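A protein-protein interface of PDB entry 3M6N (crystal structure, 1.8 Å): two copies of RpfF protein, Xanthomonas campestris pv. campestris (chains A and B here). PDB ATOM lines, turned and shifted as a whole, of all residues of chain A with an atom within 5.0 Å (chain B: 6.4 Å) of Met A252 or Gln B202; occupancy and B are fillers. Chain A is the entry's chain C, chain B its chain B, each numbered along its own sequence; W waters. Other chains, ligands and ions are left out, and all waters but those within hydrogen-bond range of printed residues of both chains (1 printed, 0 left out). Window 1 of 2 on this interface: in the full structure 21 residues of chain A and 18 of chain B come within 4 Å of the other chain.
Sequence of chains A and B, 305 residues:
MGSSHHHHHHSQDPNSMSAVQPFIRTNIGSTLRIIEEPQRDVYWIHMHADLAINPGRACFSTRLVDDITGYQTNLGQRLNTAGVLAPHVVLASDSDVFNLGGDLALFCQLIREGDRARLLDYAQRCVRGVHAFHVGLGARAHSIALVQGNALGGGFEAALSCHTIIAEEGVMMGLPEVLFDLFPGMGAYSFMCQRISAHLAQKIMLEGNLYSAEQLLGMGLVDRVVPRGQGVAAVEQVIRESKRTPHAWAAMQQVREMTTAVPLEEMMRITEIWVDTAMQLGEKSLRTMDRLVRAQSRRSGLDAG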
ATOM      1  N   ALA A 248       6.672   2.912   4.284  1.00  0.00           N
ATOM      2  CA  ALA A 248       8.009   2.597   3.798  1.00  0.00           C
ATOM      3  C   ALA A 248       8.131   1.110   3.487  1.00  0.00           C
ATOM      4  O   ALA A 248       8.772   0.718   2.511  1.00  0.00           O
ATOM      5  CB  ALA A 248       9.059   3.018   4.815  1.00  0.00           C
ATOM      6  N   TRP A 249       7.509   0.282   4.321  1.00  0.00           N
ATOM      7  CA  TRP A 249       7.511  -1.157   4.094  1.00  0.00           C
ATOM      8  C   TRP A 249       6.788  -1.503   2.798  1.00  0.00           C
ATOM      9  O   TRP A 249       7.299  -2.261   1.975  1.00  0.00           O
ATOM     10  CB  TRP A 249       6.857  -1.894   5.264  1.00  0.00           C
ATOM     11  CG  TRP A 249       6.566  -3.328   4.952  1.00  0.00           C
ATOM     12  CD1 TRP A 249       5.395  -3.843   4.480  1.00  0.00           C
ATOM     13  CD2 TRP A 249       7.471  -4.432   5.074  1.00  0.00           C
ATOM     14  NE1 TRP A 249       5.510  -5.201   4.307  1.00  0.00           N
ATOM     15  CE2 TRP A 249       6.774  -5.587   4.665  1.00  0.00           C
ATOM     16  CE3 TRP A 249       8.798  -4.556   5.493  1.00  0.00           C
ATOM     17  CZ2 TRP A 249       7.363  -6.850   4.664  1.00  0.00           C
ATOM     18  CZ3 TRP A 249       9.380  -5.812   5.490  1.00  0.00           C
ATOM     19  CH2 TRP A 249       8.662  -6.941   5.079  1.00  0.00           C
ATOM     20  N   ALA A 250       5.594  -0.944   2.626  1.00  0.00           N
ATOM     21  CA  ALA A 250       4.805  -1.187   1.425  1.00  0.00           C
ATOM     22  C   ALA A 250       5.591  -0.798   0.180  1.00  0.00           C
ATOM     23  O   ALA A 250       5.610  -1.530  -0.808  1.00  0.00           O
ATOM     24  CB  ALA A 250       3.493  -0.424   1.488  1.00  0.00           C
ATOM     25  N   ALA A 251       6.241   0.360   0.236  1.00  0.00           N
ATOM     26  CA  ALA A 251       7.058   0.833  -0.874  1.00  0.00           C
ATOM     27  C   ALA A 251       8.174  -0.159  -1.189  1.00  0.00           C
ATOM     28  O   ALA A 251       8.401  -0.504  -2.349  1.00  0.00           O
ATOM     29  CB  ALA A 251       7.634   2.203  -0.560  1.00  0.00           C
ATOM     30  N   MET A 252       8.867  -0.615  -0.150  1.00  0.00           N
ATOM     31  CA  MET A 252       9.947  -1.581  -0.321  1.00  0.00           C
ATOM     32  C   MET A 252       9.457  -2.825  -1.048  1.00  0.00           C
ATOM     33  O   MET A 252      10.137  -3.346  -1.932  1.00  0.00           O
ATOM     34  CB  MET A 252      10.542  -1.973   1.033  1.00  0.00           C
ATOM     35  CG  MET A 252      11.740  -2.915   0.936  1.00  0.00           C
ATOM     36  SD  MET A 252      13.263  -2.084   0.428  1.00  0.00           S
ATOM     37  CE  MET A 252      13.301  -0.752   1.618  1.00  0.00           C
ATOM     38  N   GLN A 253       8.275  -3.302  -0.672  1.00  0.00           N
ATOM     39  CA  GLN A 253       7.709  -4.495  -1.289  1.00  0.00           C
ATOM     40  C   GLN A 253       7.399  -4.247  -2.761  1.00  0.00           C
ATOM     41  O   GLN A 253       7.590  -5.124  -3.602  1.00  0.00           O
ATOM     42  CB  GLN A 253       6.453  -4.949  -0.542  1.00  0.00           C
ATOM     43  CG  GLN A 253       6.658  -5.114   0.956  1.00  0.00           C
ATOM     44  CD  GLN A 253       7.895  -5.928   1.287  1.00  0.00           C
ATOM     45  OE1 GLN A 253       8.764  -5.481   2.038  1.00  0.00           O
ATOM     46  NE2 GLN A 253       7.985  -7.126   0.722  1.00  0.00           N
ATOM     47  N   GLN A 254       6.922  -3.045  -3.068  1.00  0.00           N
ATOM     48  CA  GLN A 254       6.657  -2.665  -4.449  1.00  0.00           C
ATOM     49  C   GLN A 254       7.946  -2.711  -5.261  1.00  0.00           C
ATOM     50  O   GLN A 254       7.959  -3.174  -6.401  1.00  0.00           O
ATOM     51  CB  GLN A 254       6.042  -1.266  -4.522  1.00  0.00           C
ATOM     52  CG  GLN A 254       4.713  -1.125  -3.798  1.00  0.00           C
ATOM     53  CD  GLN A 254       4.090   0.242  -3.995  1.00  0.00           C
ATOM     54  OE1 GLN A 254       3.888   0.690  -5.124  1.00  0.00           O
ATOM     55  NE2 GLN A 254       3.778   0.915  -2.893  1.00  0.00           N
ATOM     56  N   VAL A 255       9.030  -2.225  -4.665  1.00  0.00           N
ATOM     57  CA  VAL A 255      10.329  -2.237  -5.325  1.00  0.00           C
ATOM     58  C   VAL A 255      10.822  -3.666  -5.534  1.00  0.00           C
ATOM     59  O   VAL A 255      11.323  -4.007  -6.603  1.00  0.00           O
ATOM     60  CB  VAL A 255      11.378  -1.435  -4.535  1.00  0.00           C
ATOM     61  CG1 VAL A 255      12.743  -1.555  -5.194  1.00  0.00           C
ATOM     62  CG2 VAL A 255      10.957   0.022  -4.430  1.00  0.00           C
ATOM     63  N   ARG A 256      10.672  -4.500  -4.508  1.00  0.00           N
ATOM     64  CA  ARG A 256      11.056  -5.906  -4.604  1.00  0.00           C
ATOM     65  C   ARG A 256      10.351  -6.581  -5.772  1.00  0.00           C
ATOM     66  O   ARG A 256      10.956  -7.343  -6.524  1.00  0.00           O
ATOM     67  CB  ARG A 256      10.714  -6.647  -3.311  1.00  0.00           C
ATOM     68  CG  ARG A 256      11.471  -6.158  -2.095  1.00  0.00           C
ATOM     69  CD  ARG A 256      11.029  -6.880  -0.832  1.00  0.00           C
ATOM     70  NE  ARG A 256      11.342  -8.306  -0.871  1.00  0.00           N
ATOM     71  CZ  ARG A 256      11.170  -9.134   0.155  1.00  0.00           C
ATOM     72  NH1 ARG A 256      10.687  -8.676   1.303  1.00  0.00           N
ATOM     73  NH2 ARG A 256      11.481 -10.416   0.034  1.00  0.00           N
ATOM     74  N   PHE B 183      10.252   6.644   2.506  1.00  0.00           N
ATOM     75  CA  PHE B 183      11.043   5.682   1.748  1.00  0.00           C
ATOM     76  C   PHE B 183      12.211   6.379   1.056  1.00  0.00           C
ATOM     77  O   PHE B 183      12.027   7.413   0.415  1.00  0.00           O
ATOM     78  CB  PHE B 183      10.161   4.968   0.720  1.00  0.00           C
ATOM     79  CG  PHE B 183      10.885   3.922  -0.078  1.00  0.00           C
ATOM     80  CD1 PHE B 183      11.161   2.682   0.471  1.00  0.00           C
ATOM     81  CD2 PHE B 183      11.283   4.176  -1.379  1.00  0.00           C
ATOM     82  CE1 PHE B 183      11.823   1.717  -0.263  1.00  0.00           C
ATOM     83  CE2 PHE B 183      11.948   3.214  -2.116  1.00  0.00           C
ATOM     84  CZ  PHE B 183      12.218   1.984  -1.556  1.00  0.00           C
ATOM     85  N   PRO B 184      13.420   5.813   1.188  1.00  0.00           N
ATOM     86  CA  PRO B 184      14.626   6.380   0.586  1.00  0.00           C
ATOM     87  C   PRO B 184      14.443   6.690  -0.897  1.00  0.00           C
ATOM     88  O   PRO B 184      14.026   5.819  -1.660  1.00  0.00           O
ATOM     89  CB  PRO B 184      15.659   5.265   0.767  1.00  0.00           C
ATOM     90  CG  PRO B 184      15.206   4.540   1.984  1.00  0.00           C
ATOM     91  CD  PRO B 184      13.704   4.580   1.944  1.00  0.00           C
ATOM     92  N   TYR B 189      18.464   1.138  -2.887  1.00  0.00           N
ATOM     93  CA  TYR B 189      18.359  -0.313  -2.951  1.00  0.00           C
ATOM     94  C   TYR B 189      19.145  -0.865  -4.134  1.00  0.00           C
ATOM     95  O   TYR B 189      19.924  -1.806  -3.989  1.00  0.00           O
ATOM     96  CB  TYR B 189      16.892  -0.738  -3.041  1.00  0.00           C
ATOM     97  CG  TYR B 189      16.684  -2.236  -3.023  1.00  0.00           C
ATOM     98  CD1 TYR B 189      17.082  -2.996  -1.932  1.00  0.00           C
ATOM     99  CD2 TYR B 189      16.080  -2.886  -4.091  1.00  0.00           C
ATOM    100  CE1 TYR B 189      16.892  -4.365  -1.909  1.00  0.00           C
ATOM    101  CE2 TYR B 189      15.885  -4.255  -4.075  1.00  0.00           C
ATOM    102  CZ  TYR B 189      16.292  -4.988  -2.982  1.00  0.00           C
ATOM    103  OH  TYR B 189      16.099  -6.350  -2.960  1.00  0.00           O
ATOM    104  N   MET B 192      22.946  -0.521  -3.468  1.00  0.00           N
ATOM    105  CA  MET B 192      23.442  -1.409  -2.420  1.00  0.00           C
ATOM    106  C   MET B 192      23.550  -2.850  -2.913  1.00  0.00           C
ATOM    107  O   MET B 192      24.486  -3.566  -2.558  1.00  0.00           O
ATOM    108  CB  MET B 192      22.561  -1.338  -1.169  1.00  0.00           C
ATOM    109  CG  MET B 192      22.599   0.005  -0.453  1.00  0.00           C
ATOM    110  SD  MET B 192      21.896  -0.051   1.211  1.00  0.00           S
ATOM    111  CE  MET B 192      23.271  -0.695   2.153  1.00  0.00           C
ATOM    112  N   ILE B 196      26.151  -5.601  -1.729  1.00  0.00           N
ATOM    113  CA  ILE B 196      25.704  -6.561  -0.727  1.00  0.00           C
ATOM    114  C   ILE B 196      24.480  -7.338  -1.198  1.00  0.00           C
ATOM    115  O   ILE B 196      23.961  -7.096  -2.287  1.00  0.00           O
ATOM    116  CB  ILE B 196      25.378  -5.867   0.608  1.00  0.00           C
ATOM    117  CG1 ILE B 196      24.286  -4.815   0.407  1.00  0.00           C
ATOM    118  CG2 ILE B 196      26.630  -5.233   1.198  1.00  0.00           C
ATOM    119  CD1 ILE B 196      23.819  -4.165   1.693  1.00  0.00           C
ATOM    120  N   SER B 197      24.024  -8.272  -0.371  1.00  0.00           N
ATOM    121  CA  SER B 197      22.868  -9.093  -0.709  1.00  0.00           C
ATOM    122  C   SER B 197      21.596  -8.257  -0.756  1.00  0.00           C
ATOM    123  O   SER B 197      21.501  -7.214  -0.108  1.00  0.00           O
ATOM    124  CB  SER B 197      22.702 -10.225   0.306  1.00  0.00           C
ATOM    125  OG  SER B 197      22.271  -9.723   1.560  1.00  0.00           O
ATOM    126  N   ALA B 198      20.618  -8.719  -1.526  1.00  0.00           N
ATOM    127  CA  ALA B 198      19.335  -8.040  -1.613  1.00  0.00           C
ATOM    128  C   ALA B 198      18.669  -7.995  -0.242  1.00  0.00           C
ATOM    129  O   ALA B 198      18.039  -7.004   0.123  1.00  0.00           O
ATOM    130  CB  ALA B 198      18.435  -8.734  -2.621  1.00  0.00           C
ATOM    131  N   HIS B 199      18.818  -9.077   0.515  1.00  0.00           N
ATOM    132  CA  HIS B 199      18.205  -9.174   1.835  1.00  0.00           C
ATOM    133  C   HIS B 199      18.782  -8.150   2.809  1.00  0.00           C
ATOM    134  O   HIS B 199      18.039  -7.446   3.496  1.00  0.00           O
ATOM    135  CB  HIS B 199      18.366 -10.585   2.401  1.00  0.00           C
ATOM    136  CG  HIS B 199      17.723 -10.771   3.738  1.00  0.00           C
ATOM    137  ND1 HIS B 199      16.374 -11.015   3.887  1.00  0.00           N
ATOM    138  CD2 HIS B 199      18.240 -10.743   4.989  1.00  0.00           C
ATOM    139  CE1 HIS B 199      16.090 -11.129   5.171  1.00  0.00           C
ATOM    140  NE2 HIS B 199      17.204 -10.970   5.862  1.00  0.00           N
ATOM    141  N   LEU B 200      20.108  -8.075   2.870  1.00  0.00           N
ATOM    142  CA  LEU B 200      20.775  -7.132   3.760  1.00  0.00           C
ATOM    143  C   LEU B 200      20.460  -5.694   3.362  1.00  0.00           C
ATOM    144  O   LEU B 200      20.277  -4.829   4.219  1.00  0.00           O
ATOM    145  CB  LEU B 200      22.288  -7.361   3.756  1.00  0.00           C
ATOM    146  CG  LEU B 200      23.101  -6.461   4.688  1.00  0.00           C
ATOM    147  CD1 LEU B 200      22.569  -6.538   6.112  1.00  0.00           C
ATOM    148  CD2 LEU B 200      24.576  -6.830   4.641  1.00  0.00           C
ATOM    149  N   ALA B 201      20.396  -5.444   2.059  1.00  0.00           N
ATOM    150  CA  ALA B 201      20.057  -4.117   1.560  1.00  0.00           C
ATOM    151  C   ALA B 201      18.699  -3.677   2.099  1.00  0.00           C
ATOM    152  O   ALA B 201      18.537  -2.545   2.554  1.00  0.00           O
ATOM    153  CB  ALA B 201      20.060  -4.101   0.040  1.00  0.00           C
ATOM    154  N   GLN B 202      17.726  -4.582   2.048  1.00  0.00           N
ATOM    155  CA  GLN B 202      16.383  -4.284   2.535  1.00  0.00           C
ATOM    156  C   GLN B 202      16.395  -3.924   4.017  1.00  0.00           C
ATOM    157  O   GLN B 202      15.797  -2.928   4.428  1.00  0.00           O
ATOM    158  CB  GLN B 202      15.444  -5.466   2.296  1.00  0.00           C
ATOM    159  CG  GLN B 202      14.036  -5.245   2.828  1.00  0.00           C
ATOM    160  CD  GLN B 202      13.081  -6.362   2.450  1.00  0.00           C
ATOM    161  OE1 GLN B 202      11.945  -6.408   2.923  1.00  0.00           O
ATOM    162  NE2 GLN B 202      13.539  -7.270   1.596  1.00  0.00           N
ATOM    163  N   LYS B 203      17.077  -4.742   4.813  1.00  0.00           N
ATOM    164  CA  LYS B 203      17.157  -4.521   6.253  1.00  0.00           C
ATOM    165  C   LYS B 203      17.770  -3.161   6.569  1.00  0.00           C
ATOM    166  O   LYS B 203      17.230  -2.399   7.370  1.00  0.00           O
ATOM    167  CB  LYS B 203      17.958  -5.639   6.924  1.00  0.00           C
ATOM    168  CG  LYS B 203      17.305  -7.008   6.821  1.00  0.00           C
ATOM    169  CD  LYS B 203      18.211  -8.105   7.358  1.00  0.00           C
ATOM    170  CE  LYS B 203      18.496  -7.916   8.837  1.00  0.00           C
ATOM    171  NZ  LYS B 203      19.326  -9.027   9.383  1.00  0.00           N
ATOM    172  N   ILE B 204      18.896  -2.860   5.931  1.00  0.00           N
ATOM    173  CA  ILE B 204      19.554  -1.570   6.108  1.00  0.00           C
ATOM    174  C   ILE B 204      18.624  -0.433   5.701  1.00  0.00           C
ATOM    175  O   ILE B 204      18.575   0.609   6.356  1.00  0.00           O
ATOM    176  CB  ILE B 204      20.841  -1.477   5.273  1.00  0.00           C
ATOM    177  CG1 ILE B 204      21.914  -2.408   5.840  1.00  0.00           C
ATOM    178  CG2 ILE B 204      21.345  -0.044   5.235  1.00  0.00           C
ATOM    179  CD1 ILE B 204      23.186  -2.442   5.021  1.00  0.00           C
ATOM    180  N   MET B 205      17.891  -0.655   4.613  1.00  0.00           N
ATOM    181  CA  MET B 205      16.946   0.322   4.074  1.00  0.00           C
ATOM    182  C   MET B 205      15.778   0.600   5.018  1.00  0.00           C
ATOM    183  O   MET B 205      15.184   1.675   4.971  1.00  0.00           O
ATOM    184  CB  MET B 205      16.388  -0.168   2.737  1.00  0.00           C
ATOM    185  CG  MET B 205      17.315  -0.011   1.536  1.00  0.00           C
ATOM    186  SD  MET B 205      17.298   1.640   0.810  1.00  0.00           S
ATOM    187  CE  MET B 205      15.660   1.716   0.089  1.00  0.00           C
ATOM    188  N   LEU B 206      15.456  -0.367   5.871  1.00  0.00           N
ATOM    189  CA  LEU B 206      14.267  -0.277   6.718  1.00  0.00           C
ATOM    190  C   LEU B 206      14.572   0.000   8.188  1.00  0.00           C
ATOM    191  O   LEU B 206      13.741   0.558   8.905  1.00  0.00           O
ATOM    192  CB  LEU B 206      13.436  -1.557   6.595  1.00  0.00           C
ATOM    193  CG  LEU B 206      12.769  -1.783   5.239  1.00  0.00           C
ATOM    194  CD1 LEU B 206      12.178  -3.180   5.152  1.00  0.00           C
ATOM    195  CD2 LEU B 206      11.703  -0.726   4.997  1.00  0.00           C
ATOM    196  N   GLU B 207      15.759  -0.396   8.637  1.00  0.00           N
ATOM    197  CA  GLU B 207      16.120  -0.268  10.048  1.00  0.00           C
ATOM    198  C   GLU B 207      16.239   1.193  10.481  1.00  0.00           C
ATOM    199  O   GLU B 207      15.841   1.554  11.589  1.00  0.00           O
ATOM    200  CB  GLU B 207      17.421  -1.020  10.340  1.00  0.00           C
ATOM    201  CG  GLU B 207      17.825  -1.030  11.807  1.00  0.00           C
ATOM    202  CD  GLU B 207      16.911  -1.884  12.662  1.00  0.00           C
ATOM    203  OE1 GLU B 207      17.028  -1.824  13.905  1.00  0.00           O
ATOM    204  OE2 GLU B 207      16.074  -2.617  12.094  1.00  0.00           O
ATOM    205  N   ILE B 273       6.939   5.140  -7.205  1.00  0.00           N
ATOM    206  CA  ILE B 273       6.669   4.509  -5.921  1.00  0.00           C
ATOM    207  C   ILE B 273       7.030   5.449  -4.777  1.00  0.00           C
ATOM    208  O   ILE B 273       6.302   5.551  -3.789  1.00  0.00           O
ATOM    209  CB  ILE B 273       7.463   3.200  -5.764  1.00  0.00           C
ATOM    210  CG1 ILE B 273       7.072   2.206  -6.859  1.00  0.00           C
ATOM    211  CG2 ILE B 273       7.237   2.601  -4.386  1.00  0.00           C
ATOM    212  CD1 ILE B 273       7.959   0.981  -6.917  1.00  0.00           C
HETATM  213  O   HOH W   1       3.948   3.927  -3.108  1.00  0.00           O
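OE1 of Gln A253 sits close to OE1 of Gln B202 (3.4 Å). NH1 of Arg A256 is in hydrogen-bond range of OE1 of Gln B202 (3.1 Å).
NE2 of Gln A253 sits close to NH1 of Arg A256 (3.2 Å).
Among the printed residues, pairs that only touch across the chains: Met A252 with Met B205 (3.3 Å), Met A252 with Phe B183 (3.4 Å), Trp A249 with Leu B206 (3.7 Å), Trp A249 with Gln B202 (3.7 Å), Val A255 with Phe B183 (3.7 Å), Ala A248 with Phe B183 (3.7 Å), Ala A251 with Phe B183 (3.7 Å), Met A252 with Leu B206 (3.7 Å), Val A255 with Tyr B189 (3.8 Å), Met A252 with Gln B202 (3.8 Å), Gln A254 with Ile B273 (3.8 Å) and Ala A251 with Ile B273 (3.9 Å).
Of chain B, only Phe B183 (3.4 Å), Gln B202 (3.8 Å), Met B205 (3.3 Å) and Leu B206 (3.7 Å) come within 4 Å of Met A252. Gln B202 touches four residues of chain A. Of the printed residues of chain B, Arg A256 touches Gln B202. Printed residues of chain B within 4 Å of Trp A249: Gln B202 and Leu B206. Of the printed residues of chain B, Ala A251 touches Phe B183 and Ile B273. Of the printed residues of chain B, Val A255 touches Phe B183 and Tyr B189. Met B192 touches none of the printed residues of chain A. Ser B197 touches none of the printed residues of chain A. The nearest printed residue of chain A that does not touch Gln B202 is Ala A248 (7.8 Å).
Of the 9 printed residues of chain A, 8 touch a printed residue of chain B. Printed residues of chain A that touch a printed residue of chain B: Ala A248, Trp A249, Ala A251, Met A252, Gln A253, Gln A254, Val A255 and Arg A256. Hydrophobic or aromatic side chains of chain A within 4 Å of the printed part of chain B: Trp A249, Ala A251, Met A252 and Val A255. Of the 17 printed residues of chain B, 6 touch a printed residue of chain A. Printed residues of chain B that touch a printed residue of chain A: Phe B183, Tyr B189, Gln B202, Met B205, Leu B206 and Ile B273.
No position is printed for both chains.
Water W1 lies within hydrogen-bond range of the backbone carbonyl oxygen of Ile B273 (2.9 Å) and the side-chain amide nitrogen of Gln A254 (3.0 Å).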
